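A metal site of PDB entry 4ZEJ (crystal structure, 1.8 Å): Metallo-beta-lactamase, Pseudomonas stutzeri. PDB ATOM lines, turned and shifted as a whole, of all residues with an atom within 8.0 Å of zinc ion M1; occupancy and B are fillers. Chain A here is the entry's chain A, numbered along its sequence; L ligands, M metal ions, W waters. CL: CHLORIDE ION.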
ATOM      1  N   HIS A  76      29.971  -9.864  20.645  1.00  0.00           N
ATOM      2  CA  HIS A  76      30.133  -9.689  19.181  1.00  0.00           C
ATOM      3  C   HIS A  76      28.759  -9.400  18.580  1.00  0.00           C
ATOM      4  O   HIS A  76      27.790  -9.346  19.315  1.00  0.00           O
ATOM      5  CB  HIS A  76      30.884 -10.855  18.478  1.00  0.00           C
ATOM      6  CG  HIS A  76      30.112 -12.118  18.351  1.00  0.00           C
ATOM      7  ND1 HIS A  76      29.966 -13.007  19.402  1.00  0.00           N
ATOM      8  CD2 HIS A  76      29.490 -12.686  17.306  1.00  0.00           C
ATOM      9  CE1 HIS A  76      29.262 -14.039  19.001  1.00  0.00           C
ATOM     10  NE2 HIS A  76      28.958 -13.873  17.739  1.00  0.00           N
ATOM     11  N   TRP A  77      28.679  -9.197  17.277  1.00  0.00           N
ATOM     12  CA  TRP A  77      27.453  -8.612  16.693  1.00  0.00           C
ATOM     13  C   TRP A  77      26.278  -9.572  16.469  1.00  0.00           C
ATOM     14  O   TRP A  77      25.151  -9.126  16.289  1.00  0.00           O
ATOM     15  CB  TRP A  77      27.771  -7.866  15.403  1.00  0.00           C
ATOM     16  CG  TRP A  77      28.065  -8.716  14.198  1.00  0.00           C
ATOM     17  CD1 TRP A  77      29.263  -9.262  13.847  1.00  0.00           C
ATOM     18  CD2 TRP A  77      27.132  -9.078  13.165  1.00  0.00           C
ATOM     19  NE1 TRP A  77      29.136  -9.951  12.655  1.00  0.00           N
ATOM     20  CE2 TRP A  77      27.845  -9.840  12.213  1.00  0.00           C
ATOM     21  CE3 TRP A  77      25.769  -8.831  12.947  1.00  0.00           C
ATOM     22  CZ2 TRP A  77      27.228 -10.385  11.074  1.00  0.00           C
ATOM     23  CZ3 TRP A  77      25.158  -9.353  11.803  1.00  0.00           C
ATOM     24  CH2 TRP A  77      25.892 -10.119  10.888  1.00  0.00           C
ATOM     25  N   HIS A  78      26.523 -10.878  16.478  1.00  0.00           N
ATOM     26  CA  HIS A  78      25.466 -11.826  16.112  1.00  0.00           C
ATOM     27  C   HIS A  78      24.302 -11.798  17.089  1.00  0.00           C
ATOM     28  O   HIS A  78      24.447 -11.374  18.237  1.00  0.00           O
ATOM     29  CB  HIS A  78      26.009 -13.259  15.975  1.00  0.00           C
ATOM     30  CG  HIS A  78      26.921 -13.438  14.802  1.00  0.00           C
ATOM     31  ND1 HIS A  78      27.902 -14.402  14.753  1.00  0.00           N
ATOM     32  CD2 HIS A  78      27.010 -12.758  13.639  1.00  0.00           C
ATOM     33  CE1 HIS A  78      28.530 -14.339  13.597  1.00  0.00           C
ATOM     34  NE2 HIS A  78      28.019 -13.341  12.906  1.00  0.00           N
ATOM     35  N   GLU A  79      23.154 -12.283  16.617  1.00  0.00           N
ATOM     36  CA  GLU A  79      21.883 -12.162  17.340  1.00  0.00           C
ATOM     37  C   GLU A  79      21.847 -12.830  18.712  1.00  0.00           C
ATOM     38  O   GLU A  79      21.144 -12.348  19.621  1.00  0.00           O
ATOM     39  CB  GLU A  79      20.724 -12.693  16.486  1.00  0.00           C
ATOM     40  CG  GLU A  79      20.391 -11.790  15.317  1.00  0.00           C
ATOM     41  CD  GLU A  79      19.249 -12.296  14.455  1.00  0.00           C
ATOM     42  OE1 GLU A  79      18.375 -13.053  14.963  1.00  0.00           O
ATOM     43  OE2 GLU A  79      19.199 -11.930  13.263  1.00  0.00           O
ATOM     44  N   ASP A  80      22.599 -13.920  18.886  1.00  0.00           N
ATOM     45  CA  ASP A  80      22.664 -14.560  20.219  1.00  0.00           C
ATOM     46  C   ASP A  80      23.337 -13.675  21.281  1.00  0.00           C
ATOM     47  O   ASP A  80      23.197 -13.952  22.465  1.00  0.00           O
ATOM     48  CB  ASP A  80      23.300 -15.965  20.172  1.00  0.00           C
ATOM     49  CG  ASP A  80      24.744 -15.961  19.730  1.00  0.00           C
ATOM     50  OD1 ASP A  80      25.070 -15.275  18.762  1.00  0.00           O
ATOM     51  OD2 ASP A  80      25.563 -16.684  20.324  1.00  0.00           O
ATOM     52  N   ARG A  81      24.045 -12.622  20.869  1.00  0.00           N
ATOM     53  CA  ARG A  81      24.653 -11.648  21.799  1.00  0.00           C
ATOM     54  C   ARG A  81      23.906 -10.304  21.913  1.00  0.00           C
ATOM     55  O   ARG A  81      24.080  -9.579  22.904  1.00  0.00           O
ATOM     56  CB  ARG A  81      26.068 -11.308  21.311  1.00  0.00           C
ATOM     57  CG  ARG A  81      26.999 -12.440  20.955  1.00  0.00           C
ATOM     58  CD  ARG A  81      27.435 -13.248  22.162  1.00  0.00           C
ATOM     59  NE  ARG A  81      26.708 -14.488  22.262  1.00  0.00           N
ATOM     60  CZ  ARG A  81      26.609 -15.250  23.349  1.00  0.00           C
ATOM     61  NH1 ARG A  81      27.166 -14.909  24.526  1.00  0.00           N
ATOM     62  NH2 ARG A  81      25.927 -16.377  23.269  1.00  0.00           N
ATOM     63  N   HIS A 138      36.189 -16.330  16.245  1.00  0.00           N
ATOM     64  CA  HIS A 138      34.838 -16.598  15.808  1.00  0.00           C
ATOM     65  C   HIS A 138      34.353 -15.553  14.798  1.00  0.00           C
ATOM     66  O   HIS A 138      33.714 -15.905  13.783  1.00  0.00           O
ATOM     67  CB  HIS A 138      33.901 -16.650  17.022  1.00  0.00           C
ATOM     68  CG  HIS A 138      32.468 -16.750  16.662  1.00  0.00           C
ATOM     69  ND1 HIS A 138      31.932 -17.900  16.131  1.00  0.00           N
ATOM     70  CD2 HIS A 138      31.459 -15.856  16.730  1.00  0.00           C
ATOM     71  CE1 HIS A 138      30.658 -17.704  15.874  1.00  0.00           C
ATOM     72  NE2 HIS A 138      30.347 -16.469  16.222  1.00  0.00           N
ATOM     73  N   THR A 139      34.620 -14.291  15.102  1.00  0.00           N
ATOM     74  CA  THR A 139      34.411 -13.176  14.181  1.00  0.00           C
ATOM     75  C   THR A 139      35.566 -12.193  14.340  1.00  0.00           C
ATOM     76  O   THR A 139      36.383 -12.312  15.275  1.00  0.00           O
ATOM     77  CB  THR A 139      33.118 -12.403  14.466  1.00  0.00           C
ATOM     78  OG1 THR A 139      33.132 -11.961  15.837  1.00  0.00           O
ATOM     79  CG2 THR A 139      31.877 -13.265  14.193  1.00  0.00           C
ATOM     80  N   ASP A 141      35.173  -9.119  15.260  1.00  0.00           N
ATOM     81  CA  ASP A 141      34.862  -8.187  16.355  1.00  0.00           C
ATOM     82  C   ASP A 141      34.861  -8.808  17.761  1.00  0.00           C
ATOM     83  O   ASP A 141      34.721  -8.083  18.743  1.00  0.00           O
ATOM     84  CB  ASP A 141      33.549  -7.442  16.108  1.00  0.00           C
ATOM     85  CG  ASP A 141      32.343  -8.354  16.107  1.00  0.00           C
ATOM     86  OD1 ASP A 141      31.271  -7.944  16.641  1.00  0.00           O
ATOM     87  OD2 ASP A 141      32.449  -9.474  15.581  1.00  0.00           O
ATOM     88  N   ASN A 142      34.998 -10.125  17.872  1.00  0.00           N
ATOM     89  CA  ASN A 142      34.818 -10.784  19.174  1.00  0.00           C
ATOM     90  C   ASN A 142      35.714 -10.239  20.303  1.00  0.00           C
ATOM     91  O   ASN A 142      36.910 -10.043  20.112  1.00  0.00           O
ATOM     92  CB  ASN A 142      34.838 -12.335  19.090  1.00  0.00           C
ATOM     93  CG  ASN A 142      36.101 -12.942  18.483  1.00  0.00           C
ATOM     94  OD1 ASN A 142      36.026 -14.077  18.012  1.00  0.00           O
ATOM     95  ND2 ASN A 142      37.242 -12.272  18.525  1.00  0.00           N
ATOM     96  N   CYS A 157      31.528 -16.392  22.337  1.00  0.00           N
ATOM     97  CA  CYS A 157      31.602 -17.407  21.294  1.00  0.00           C
ATOM     98  C   CYS A 157      33.027 -17.573  20.743  1.00  0.00           C
ATOM     99  O   CYS A 157      33.305 -18.489  19.970  1.00  0.00           O
ATOM    100  CB  CYS A 157      30.548 -17.113  20.242  1.00  0.00           C
ATOM    101  SG  CYS A 157      28.955 -16.853  21.068  1.00  0.00           S
ATOM    102  N   PHE A 158      33.933 -16.697  21.177  1.00  0.00           N
ATOM    103  CA  PHE A 158      35.374 -16.888  20.996  1.00  0.00           C
ATOM    104  C   PHE A 158      35.928 -18.157  21.695  1.00  0.00           C
ATOM    105  O   PHE A 158      36.975 -18.684  21.292  1.00  0.00           O
ATOM    106  CB  PHE A 158      36.102 -15.628  21.513  1.00  0.00           C
ATOM    107  CG  PHE A 158      37.594 -15.681  21.434  1.00  0.00           C
ATOM    108  CD1 PHE A 158      38.363 -15.943  22.561  1.00  0.00           C
ATOM    109  CD2 PHE A 158      38.245 -15.451  20.236  1.00  0.00           C
ATOM    110  CE1 PHE A 158      39.741 -15.976  22.488  1.00  0.00           C
ATOM    111  CE2 PHE A 158      39.629 -15.495  20.144  1.00  0.00           C
ATOM    112  CZ  PHE A 158      40.377 -15.751  21.271  1.00  0.00           C
ATOM    113  N   TYR A 169      29.688 -22.238  14.028  1.00  0.00           N
ATOM    114  CA  TYR A 169      29.505 -21.496  12.764  1.00  0.00           C
ATOM    115  C   TYR A 169      30.793 -20.749  12.407  1.00  0.00           C
ATOM    116  O   TYR A 169      31.193 -19.844  13.147  1.00  0.00           O
ATOM    117  CB  TYR A 169      28.330 -20.506  12.877  1.00  0.00           C
ATOM    118  CG  TYR A 169      28.256 -19.553  11.689  1.00  0.00           C
ATOM    119  CD1 TYR A 169      27.898 -20.009  10.425  1.00  0.00           C
ATOM    120  CD2 TYR A 169      28.567 -18.212  11.836  1.00  0.00           C
ATOM    121  CE1 TYR A 169      27.827 -19.136   9.335  1.00  0.00           C
ATOM    122  CE2 TYR A 169      28.512 -17.334  10.764  1.00  0.00           C
ATOM    123  CZ  TYR A 169      28.138 -17.794   9.519  1.00  0.00           C
ATOM    124  OH  TYR A 169      28.094 -16.903   8.461  1.00  0.00           O
ATOM    125  N   GLU A 172      32.191 -16.631   9.230  1.00  0.00           N
ATOM    126  CA  GLU A 172      32.839 -15.343   9.410  1.00  0.00           C
ATOM    127  C   GLU A 172      34.129 -15.435  10.255  1.00  0.00           C
ATOM    128  O   GLU A 172      34.665 -14.419  10.685  1.00  0.00           O
ATOM    129  CB  GLU A 172      31.822 -14.351  10.013  1.00  0.00           C
ATOM    130  CG  GLU A 172      30.693 -14.054   9.034  1.00  0.00           C
ATOM    131  CD  GLU A 172      29.382 -13.606   9.669  1.00  0.00           C
ATOM    132  OE1 GLU A 172      29.416 -12.887  10.675  1.00  0.00           O
ATOM    133  OE2 GLU A 172      28.292 -13.952   9.119  1.00  0.00           O
ATOM    134  N   HIS A 199      28.385 -20.819  24.380  1.00  0.00           N
ATOM    135  CA  HIS A 199      27.457 -21.952  24.270  1.00  0.00           C
ATOM    136  C   HIS A 199      28.034 -23.147  25.010  1.00  0.00           C
ATOM    137  O   HIS A 199      29.202 -23.455  24.851  1.00  0.00           O
ATOM    138  CB  HIS A 199      27.276 -22.333  22.805  1.00  0.00           C
ATOM    139  CG  HIS A 199      26.821 -21.196  21.948  1.00  0.00           C
ATOM    140  ND1 HIS A 199      25.501 -20.805  21.881  1.00  0.00           N
ATOM    141  CD2 HIS A 199      27.518 -20.348  21.162  1.00  0.00           C
ATOM    142  CE1 HIS A 199      25.401 -19.772  21.067  1.00  0.00           C
ATOM    143  NE2 HIS A 199      26.609 -19.473  20.607  1.00  0.00           N
HETATM  144 CL    CL L   1      27.311 -16.903  17.670  1.00  0.00          CL
HETATM  145 ZN    ZN M   1      28.520 -15.490  16.380  1.00  0.00          ZN
HETATM  146 ZN    ZN M   2      27.306 -17.599  19.829  1.00  0.00          ZN
HETATM  147  O   HOH W   1      27.512 -17.352  15.000  1.00  0.00           O
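NE2 of His 78 lies within hydrogen-bond range of OE1 of Glu 172 (2.7 Å).
The backbone NH (N) of His 138 sits at hydrogen-bond distance from the side-chain amide oxygen (OD1) of Asn 142, at 2.9 Å.
Within 4 Å of zinc ion M1: His 76, His 78 and His 138.
The nearest printed residue that does not touch zinc ion M1 is Asp 80 (4.2 Å).
Zinc ion M1 is bound by ND1 of His 78 (2.1 Å), NE2 of His 138 (2.1 Å), NE2 of His 76 (2.2 Å), CL of the ligand (2.3 Å) and water W1 (2.5 Å).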
